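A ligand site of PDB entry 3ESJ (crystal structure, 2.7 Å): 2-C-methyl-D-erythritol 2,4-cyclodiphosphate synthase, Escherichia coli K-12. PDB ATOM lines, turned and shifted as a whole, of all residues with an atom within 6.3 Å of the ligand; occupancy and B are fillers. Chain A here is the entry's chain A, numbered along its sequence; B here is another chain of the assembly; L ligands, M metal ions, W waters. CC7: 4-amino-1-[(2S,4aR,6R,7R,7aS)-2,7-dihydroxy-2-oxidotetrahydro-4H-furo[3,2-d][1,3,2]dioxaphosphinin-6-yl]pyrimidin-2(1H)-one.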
ATOM      1  N   ILE A 104       8.929   1.382  -1.531  1.00  0.00           N
ATOM      2  CA  ILE A 104       9.860   1.690  -2.609  1.00  0.00           C
ATOM      3  C   ILE A 104       9.077   1.770  -3.917  1.00  0.00           C
ATOM      4  O   ILE A 104       8.257   0.896  -4.214  1.00  0.00           O
ATOM      5  CB  ILE A 104      10.953   0.623  -2.700  1.00  0.00           C
ATOM      6  CG1 ILE A 104      11.584   0.412  -1.317  1.00  0.00           C
ATOM      7  CG2 ILE A 104      12.023   0.984  -3.786  1.00  0.00           C
ATOM      8  CD1 ILE A 104      12.380  -0.854  -1.163  1.00  0.00           C
ATOM      9  N   ILE A 105       9.291   2.835  -4.685  1.00  0.00           N
ATOM     10  CA  ILE A 105       8.615   2.954  -5.963  1.00  0.00           C
ATOM     11  C   ILE A 105       9.668   2.892  -7.038  1.00  0.00           C
ATOM     12  O   ILE A 105      10.433   3.829  -7.209  1.00  0.00           O
ATOM     13  CB  ILE A 105       7.830   4.269  -6.057  1.00  0.00           C
ATOM     14  CG1 ILE A 105       6.759   4.276  -4.985  1.00  0.00           C
ATOM     15  CG2 ILE A 105       7.196   4.401  -7.443  1.00  0.00           C
ATOM     16  CD1 ILE A 105       6.547   5.580  -4.370  1.00  0.00           C
ATOM     17  N   ALA A 106       9.713   1.765  -7.748  1.00  0.00           N
ATOM     18  CA  ALA A 106      10.764   1.486  -8.718  1.00  0.00           C
ATOM     19  C   ALA A 106      10.271   0.493  -9.747  1.00  0.00           C
ATOM     20  O   ALA A 106       9.561  -0.486  -9.418  1.00  0.00           O
ATOM     21  CB  ALA A 106      11.995   0.924  -8.005  1.00  0.00           C
ATOM     22  N   GLN A 107      10.636   0.759 -11.003  1.00  0.00           N
ATOM     23  CA  GLN A 107      10.366  -0.175 -12.109  1.00  0.00           C
ATOM     24  C   GLN A 107      11.253  -1.411 -12.000  1.00  0.00           C
ATOM     25  O   GLN A 107      10.822  -2.517 -12.332  1.00  0.00           O
ATOM     26  CB  GLN A 107      10.601   0.543 -13.435  1.00  0.00           C
ATOM     27  CG  GLN A 107      10.134  -0.232 -14.659  1.00  0.00           C
ATOM     28  CD  GLN A 107       8.623  -0.461 -14.691  1.00  0.00           C
ATOM     29  OE1 GLN A 107       7.827   0.350 -14.203  1.00  0.00           O
ATOM     30  NE2 GLN A 107       8.223  -1.585 -15.272  1.00  0.00           N
ATOM     31  N   ALA A 108      12.492  -1.202 -11.551  1.00  0.00           N
ATOM     32  CA  ALA A 108      13.542  -2.208 -11.464  1.00  0.00           C
ATOM     33  C   ALA A 108      14.657  -1.574 -10.664  1.00  0.00           C
ATOM     34  O   ALA A 108      14.769  -0.357 -10.666  1.00  0.00           O
ATOM     35  CB  ALA A 108      14.046  -2.581 -12.866  1.00  0.00           C
ATOM     36  N   PRO A 109      15.512  -2.376 -10.002  1.00  0.00           N
ATOM     37  CA  PRO A 109      15.562  -3.843  -9.921  1.00  0.00           C
ATOM     38  C   PRO A 109      14.472  -4.421  -9.019  1.00  0.00           C
ATOM     39  O   PRO A 109      13.782  -3.633  -8.351  1.00  0.00           O
ATOM     40  CB  PRO A 109      16.945  -4.112  -9.312  1.00  0.00           C
ATOM     41  CG  PRO A 109      17.259  -2.852  -8.545  1.00  0.00           C
ATOM     42  CD  PRO A 109      16.613  -1.734  -9.258  1.00  0.00           C
ATOM     43  N   LYS A 110      14.316  -5.754  -8.990  1.00  0.00           N
ATOM     44  CA  LYS A 110      13.367  -6.415  -8.080  1.00  0.00           C
ATOM     45  C   LYS A 110      13.741  -6.144  -6.624  1.00  0.00           C
ATOM     46  O   LYS A 110      14.890  -6.339  -6.250  1.00  0.00           O
ATOM     47  CB  LYS A 110      13.363  -7.933  -8.282  1.00  0.00           C
ATOM     48  CG  LYS A 110      12.210  -8.439  -9.075  1.00  0.00           C
ATOM     49  CD  LYS A 110      10.909  -8.671  -8.247  1.00  0.00           C
ATOM     50  CE  LYS A 110       9.757  -8.985  -9.221  1.00  0.00           C
ATOM     51  NZ  LYS A 110       8.370  -8.793  -8.705  1.00  0.00           N
ATOM     52  N   MET A 111      12.768  -5.732  -5.808  1.00  0.00           N
ATOM     53  CA  MET A 111      13.044  -5.363  -4.419  1.00  0.00           C
ATOM     54  C   MET A 111      12.717  -6.499  -3.463  1.00  0.00           C
ATOM     55  O   MET A 111      13.413  -6.704  -2.462  1.00  0.00           O
ATOM     56  CB  MET A 111      12.282  -4.116  -4.010  1.00  0.00           C
ATOM     57  CG  MET A 111      12.689  -2.884  -4.794  1.00  0.00           C
ATOM     58  SD  MET A 111      14.409  -2.422  -4.464  1.00  0.00           S
ATOM     59  CE  MET A 111      14.619  -1.131  -5.675  1.00  0.00           C
ATOM     60  N   LEU A 112      11.677  -7.259  -3.807  1.00  0.00           N
ATOM     61  CA  LEU A 112      11.207  -8.354  -2.953  1.00  0.00           C
ATOM     62  C   LEU A 112      12.281  -9.264  -2.322  1.00  0.00           C
ATOM     63  O   LEU A 112      12.190  -9.555  -1.127  1.00  0.00           O
ATOM     64  CB  LEU A 112      10.153  -9.196  -3.668  1.00  0.00           C
ATOM     65  CG  LEU A 112       8.711  -8.824  -3.393  1.00  0.00           C
ATOM     66  CD1 LEU A 112       7.854  -9.561  -4.401  1.00  0.00           C
ATOM     67  CD2 LEU A 112       8.270  -9.153  -1.951  1.00  0.00           C
ATOM     68  N   PRO A 113      13.275  -9.747  -3.121  1.00  0.00           N
ATOM     69  CA  PRO A 113      14.266 -10.627  -2.511  1.00  0.00           C
ATOM     70  C   PRO A 113      15.096  -9.970  -1.416  1.00  0.00           C
ATOM     71  O   PRO A 113      15.613 -10.664  -0.523  1.00  0.00           O
ATOM     72  CB  PRO A 113      15.181 -11.006  -3.692  1.00  0.00           C
ATOM     73  CG  PRO A 113      14.334 -10.807  -4.897  1.00  0.00           C
ATOM     74  CD  PRO A 113      13.508  -9.604  -4.567  1.00  0.00           C
ATOM     75  N   ILE A 115      14.094  -7.503   0.689  1.00  0.00           N
ATOM     76  CA  ILE A 115      13.303  -6.892   1.746  1.00  0.00           C
ATOM     77  C   ILE A 115      13.618  -7.440   3.142  1.00  0.00           C
ATOM     78  O   ILE A 115      13.767  -6.655   4.074  1.00  0.00           O
ATOM     79  CB  ILE A 115      11.793  -6.825   1.401  1.00  0.00           C
ATOM     80  CG1 ILE A 115      11.568  -5.605   0.495  1.00  0.00           C
ATOM     81  CG2 ILE A 115      10.944  -6.763   2.649  1.00  0.00           C
ATOM     82  CD1 ILE A 115      10.239  -5.555  -0.195  1.00  0.00           C
ATOM     83  N   LYS A 136       7.860  -2.476   1.568  1.00  0.00           N
ATOM     84  CA  LYS A 136       7.216  -3.013   0.380  1.00  0.00           C
ATOM     85  C   LYS A 136       7.678  -2.295  -0.887  1.00  0.00           C
ATOM     86  O   LYS A 136       8.376  -1.286  -0.796  1.00  0.00           O
ATOM     87  CB  LYS A 136       5.702  -2.972   0.526  1.00  0.00           C
ATOM     88  CG  LYS A 136       5.122  -1.604   0.532  1.00  0.00           C
ATOM     89  CD  LYS A 136       3.701  -1.615   1.079  1.00  0.00           C
ATOM     90  CE  LYS A 136       3.692  -1.176   2.505  1.00  0.00           C
ATOM     91  NZ  LYS A 136       4.140   0.252   2.654  1.00  0.00           N
ATOM     92  N   ALA A 137       7.297  -2.815  -2.047  1.00  0.00           N
ATOM     93  CA  ALA A 137       7.616  -2.153  -3.288  1.00  0.00           C
ATOM     94  C   ALA A 137       6.423  -2.109  -4.235  1.00  0.00           C
ATOM     95  O   ALA A 137       5.549  -3.000  -4.216  1.00  0.00           O
ATOM     96  CB  ALA A 137       8.787  -2.825  -3.944  1.00  0.00           C
ATOM     97  N   THR A 138       6.375  -1.052  -5.036  1.00  0.00           N
ATOM     98  CA  THR A 138       5.425  -0.994  -6.154  1.00  0.00           C
ATOM     99  C   THR A 138       6.133  -0.451  -7.378  1.00  0.00           C
ATOM    100  O   THR A 138       7.071   0.353  -7.288  1.00  0.00           O
ATOM    101  CB  THR A 138       4.078  -0.249  -5.844  1.00  0.00           C
ATOM    102  OG1 THR A 138       4.113   1.084  -6.323  1.00  0.00           O
ATOM    103  CG2 THR A 138       3.798  -0.177  -4.370  1.00  0.00           C
ATOM    104  N   THR A 139       5.680  -0.935  -8.519  1.00  0.00           N
ATOM    105  CA  THR A 139       6.133  -0.472  -9.812  1.00  0.00           C
ATOM    106  C   THR A 139       5.073   0.506 -10.294  1.00  0.00           C
ATOM    107  O   THR A 139       3.954   0.436  -9.850  1.00  0.00           O
ATOM    108  CB  THR A 139       6.296  -1.642 -10.791  1.00  0.00           C
ATOM    109  OG1 THR A 139       5.755  -1.260 -12.052  1.00  0.00           O
ATOM    110  CG2 THR A 139       5.496  -2.873 -10.350  1.00  0.00           C
ATOM    111  N   GLU A 141       4.220   0.674 -13.524  1.00  0.00           N
ATOM    112  CA  GLU A 141       3.805   0.105 -14.792  1.00  0.00           C
ATOM    113  C   GLU A 141       4.325   0.896 -15.988  1.00  0.00           C
ATOM    114  O   GLU A 141       3.550   1.200 -16.906  1.00  0.00           O
ATOM    115  CB  GLU A 141       2.276   0.002 -14.890  1.00  0.00           C
ATOM    116  CG  GLU A 141       1.569  -0.626 -13.682  1.00  0.00           C
ATOM    117  CD  GLU A 141       1.765  -2.122 -13.568  1.00  0.00           C
ATOM    118  OE1 GLU A 141       0.891  -2.797 -12.987  1.00  0.00           O
ATOM    119  OE2 GLU A 141       2.812  -2.633 -14.038  1.00  0.00           O
ATOM    120  N   ASP B  14      -0.157   2.877  -5.265  1.00  0.00           N
ATOM    121  CA  ASP B  14      -0.291   2.046  -6.462  1.00  0.00           C
ATOM    122  C   ASP B  14      -0.539   2.869  -7.728  1.00  0.00           C
ATOM    123  O   ASP B  14      -1.066   3.999  -7.656  1.00  0.00           O
ATOM    124  CB  ASP B  14      -1.396   1.012  -6.263  1.00  0.00           C
ATOM    125  CG  ASP B  14      -1.411  -0.056  -7.335  1.00  0.00           C
ATOM    126  OD1 ASP B  14      -0.370  -0.243  -7.987  1.00  0.00           O
ATOM    127  OD2 ASP B  14      -2.464  -0.698  -7.545  1.00  0.00           O
ATOM    128  N   ASP B  52      -2.343  -2.561   0.601  1.00  0.00           N
ATOM    129  CA  ASP B  52      -0.945  -2.413   0.988  1.00  0.00           C
ATOM    130  C   ASP B  52      -0.784  -1.617   2.283  1.00  0.00           C
ATOM    131  O   ASP B  52       0.080  -1.953   3.096  1.00  0.00           O
ATOM    132  CB  ASP B  52      -0.129  -1.755  -0.138  1.00  0.00           C
ATOM    133  CG  ASP B  52       0.462  -2.752  -1.108  1.00  0.00           C
ATOM    134  OD1 ASP B  52       0.207  -3.974  -0.926  1.00  0.00           O
ATOM    135  OD2 ASP B  52       1.183  -2.323  -2.054  1.00  0.00           O
ATOM    136  N   ASP B  62       3.134  -6.895   1.512  1.00  0.00           N
ATOM    137  CA  ASP B  62       2.285  -6.221   0.524  1.00  0.00           C
ATOM    138  C   ASP B  62       1.581  -7.266  -0.363  1.00  0.00           C
ATOM    139  O   ASP B  62       1.870  -8.458  -0.247  1.00  0.00           O
ATOM    140  CB  ASP B  62       3.099  -5.292  -0.376  1.00  0.00           C
ATOM    141  CG  ASP B  62       4.007  -6.055  -1.317  1.00  0.00           C
ATOM    142  OD1 ASP B  62       3.726  -6.112  -2.533  1.00  0.00           O
ATOM    143  OD2 ASP B  62       4.985  -6.617  -0.808  1.00  0.00           O
ATOM    144  N   ILE B  63       0.678  -6.785  -1.250  1.00  0.00           N
ATOM    145  CA  ILE B  63      -0.087  -7.649  -2.162  1.00  0.00           C
ATOM    146  C   ILE B  63       0.788  -8.486  -3.076  1.00  0.00           C
ATOM    147  O   ILE B  63       0.445  -9.626  -3.349  1.00  0.00           O
ATOM    148  CB  ILE B  63      -1.096  -6.889  -3.035  1.00  0.00           C
ATOM    149  CG1 ILE B  63      -0.431  -5.679  -3.708  1.00  0.00           C
ATOM    150  CG2 ILE B  63      -2.305  -6.493  -2.265  1.00  0.00           C
ATOM    151  CD1 ILE B  63      -1.129  -5.199  -4.924  1.00  0.00           C
ATOM    152  N   GLY B  64       1.901  -7.940  -3.566  1.00  0.00           N
ATOM    153  CA  GLY B  64       2.817  -8.673  -4.462  1.00  0.00           C
ATOM    154  C   GLY B  64       3.448  -9.895  -3.809  1.00  0.00           C
ATOM    155  O   GLY B  64       3.776 -10.879  -4.481  1.00  0.00           O
ATOM    156  N   LYS B  65       3.638  -9.824  -2.505  1.00  0.00           N
ATOM    157  CA  LYS B  65       4.105 -10.954  -1.750  1.00  0.00           C
ATOM    158  C   LYS B  65       2.976 -11.936  -1.444  1.00  0.00           C
ATOM    159  O   LYS B  65       3.166 -13.142  -1.610  1.00  0.00           O
ATOM    160  CB  LYS B  65       4.832 -10.472  -0.478  1.00  0.00           C
ATOM    161  CG  LYS B  65       4.851 -11.450   0.657  1.00  0.00           C
ATOM    162  CD  LYS B  65       6.207 -11.524   1.277  1.00  0.00           C
ATOM    163  CE  LYS B  65       6.176 -12.401   2.528  1.00  0.00           C
ATOM    164  NZ  LYS B  65       5.806 -11.581   3.721  1.00  0.00           N
ATOM    165  N   PHE B  67      -0.094 -12.100  -3.004  1.00  0.00           N
ATOM    166  CA  PHE B  67      -0.786 -12.516  -4.224  1.00  0.00           C
ATOM    167  C   PHE B  67       0.099 -12.313  -5.467  1.00  0.00           C
ATOM    168  O   PHE B  67      -0.079 -11.338  -6.201  1.00  0.00           O
ATOM    169  CB  PHE B  67      -2.130 -11.780  -4.388  1.00  0.00           C
ATOM    170  CG  PHE B  67      -2.915 -11.605  -3.103  1.00  0.00           C
ATOM    171  CD1 PHE B  67      -3.115 -10.334  -2.556  1.00  0.00           C
ATOM    172  CD2 PHE B  67      -3.459 -12.697  -2.443  1.00  0.00           C
ATOM    173  CE1 PHE B  67      -3.836 -10.167  -1.371  1.00  0.00           C
ATOM    174  CE2 PHE B  67      -4.180 -12.529  -1.257  1.00  0.00           C
ATOM    175  CZ  PHE B  67      -4.367 -11.267  -0.727  1.00  0.00           C
ATOM    176  N   PRO B  68       1.064 -13.244  -5.709  1.00  0.00           N
ATOM    177  CA  PRO B  68       2.028 -13.178  -6.807  1.00  0.00           C
ATOM    178  C   PRO B  68       1.436 -12.974  -8.223  1.00  0.00           C
ATOM    179  O   PRO B  68       0.452 -13.644  -8.603  1.00  0.00           O
ATOM    180  CB  PRO B  68       2.747 -14.538  -6.727  1.00  0.00           C
ATOM    181  CG  PRO B  68       2.636 -14.932  -5.303  1.00  0.00           C
ATOM    182  CD  PRO B  68       1.270 -14.459  -4.892  1.00  0.00           C
ATOM    183  N   ASP B  69       2.073 -12.066  -8.979  1.00  0.00           N
ATOM    184  CA  ASP B  69       1.881 -11.887 -10.437  1.00  0.00           C
ATOM    185  C   ASP B  69       1.917 -13.189 -11.243  1.00  0.00           C
ATOM    186  O   ASP B  69       1.246 -13.319 -12.270  1.00  0.00           O
ATOM    187  CB  ASP B  69       2.997 -10.970 -10.983  1.00  0.00           C
ATOM    188  CG  ASP B  69       2.473  -9.627 -11.428  1.00  0.00           C
ATOM    189  OD1 ASP B  69       1.238  -9.419 -11.427  1.00  0.00           O
ATOM    190  OD2 ASP B  69       3.306  -8.768 -11.784  1.00  0.00           O
HETATM  191  O2  CC7 L   1       9.778  -6.458  -5.993  1.00  0.00           O
HETATM  192  C2  CC7 L   1       9.418  -5.454  -6.575  1.00  0.00           C
HETATM  193  N3  CC7 L   1      10.301  -4.594  -7.088  1.00  0.00           N
HETATM  194  C4  CC7 L   1       9.890  -3.488  -7.718  1.00  0.00           C
HETATM  195  N4  CC7 L   1      10.788  -2.678  -8.195  1.00  0.00           N
HETATM  196  C5  CC7 L   1       8.543  -3.208  -7.891  1.00  0.00           C
HETATM  197  C6  CC7 L   1       7.599  -4.092  -7.391  1.00  0.00           C
HETATM  198  N1  CC7 L   1       8.067  -5.238  -6.718  1.00  0.00           N
HETATM  199  C1' CC7 L   1       7.170  -6.228  -6.154  1.00  0.00           C
HETATM  200  O4' CC7 L   1       6.838  -7.032  -7.300  1.00  0.00           O
HETATM  201  C4' CC7 L   1       5.514  -7.410  -7.124  1.00  0.00           C
HETATM  202  C5' CC7 L   1       4.845  -7.714  -8.456  1.00  0.00           C
HETATM  203  O5' CC7 L   1       3.424  -7.806  -8.276  1.00  0.00           O
HETATM  204  P   CC7 L   1       2.632  -6.637  -7.465  1.00  0.00           P
HETATM  205  O2P CC7 L   1       2.775  -5.319  -8.318  1.00  0.00           O
HETATM  206  O1P CC7 L   1       1.255  -7.061  -7.135  1.00  0.00           O
HETATM  207  O3' CC7 L   1       3.561  -6.281  -6.268  1.00  0.00           O
HETATM  208  C3' CC7 L   1       4.907  -6.082  -6.684  1.00  0.00           C
HETATM  209  C2' CC7 L   1       5.862  -5.708  -5.586  1.00  0.00           C
HETATM  210  O2' CC7 L   1       5.575  -6.493  -4.438  1.00  0.00           O
HETATM  211 ZN    ZN M   1      -2.344  -2.498  -8.484  1.00  0.00          ZN
HETATM  212  O   HOH W   1      -1.597  -8.884  -7.237  1.00  0.00           O
HETATM  213  O   HOH W   2       8.137  -6.137 -10.421  1.00  0.00           O
HETATM  214  O   HOH W   3       5.500 -10.648  -7.303  1.00  0.00           O
HETATM  215  O   HOH W   4       7.087  -5.623  -2.207  1.00  0.00           O
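The backbone NH (N) of Leu 112 sits at hydrogen-bond distance from an oxygen (O2) of the ligand, at 3.0 Å.
The backbone NH (N) of Met 111 sits at hydrogen-bond distance from a nitrogen (N3) of the ligand, at 3.0 Å.
The backbone carbonyl oxygen of Ala 106 sits at hydrogen-bond distance from a nitrogen (N4) of the ligand, 2.8 Å away.
An oxygen (O2') of the ligand lies within hydrogen-bond range of the side-chain carboxylate of Asp 62 of chain B (2.7 Å).
The side-chain amino group of Lys 110 lies within hydrogen-bond range of an oxygen (O4') of the ligand.
The backbone carbonyl oxygen of Pro 109 sits at hydrogen-bond distance from a nitrogen (N4) of the ligand (3.1 Å).
The side-chain hydroxyl (OG1) of Thr 139 is in hydrogen-bond range of the side-chain amide oxygen (OE1) of Gln 107 (3.4 Å).
The side-chain carboxylate (OD1) of Asp 62 of chain B lies within hydrogen-bond range of the backbone NH (N) of Gly 64 of chain B (2.8 Å).
N of Ile 63 of chain B lies within hydrogen-bond range of OD1 of Asp 52 of chain B.
N of Glu 141 is in hydrogen-bond range of OG1 of Thr 139, at 2.9 Å.
The backbone NH of Thr 138 is in hydrogen-bond range of the backbone carbonyl oxygen of Ile 104.
N of Ala 106 sits at hydrogen-bond distance from O of Thr 138 (3.0 Å).
O of Ala 137 touches C2' of the ligand (3.1 Å).
C of Thr 138 touches C5 of the ligand, 3.7 Å away.
N of Thr 139 touches C5 of the ligand, 3.7 Å away.
Ile 63 of chain B touches the ligand.
CA of Gly 64 of chain B touches O3' of the ligand (3.1 Å).
Asp 69 of chain B touches the ligand.
Hydrophobic or aromatic side chains within 4 Å of the ligand: Ala 106, Met 111, Leu 112, Ala 137 and Ile 63 of chain B.
Water W4 lies within hydrogen-bond range of the side-chain carboxylate of Asp 62 of chain B, the backbone NH of Ala 137 and an oxygen (O2') of the ligand.
Water W2 lies within hydrogen-bond range of the side-chain amino group of Lys 110 (3.2 Å) and an oxygen (O4') of the ligand (3.5 Å).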
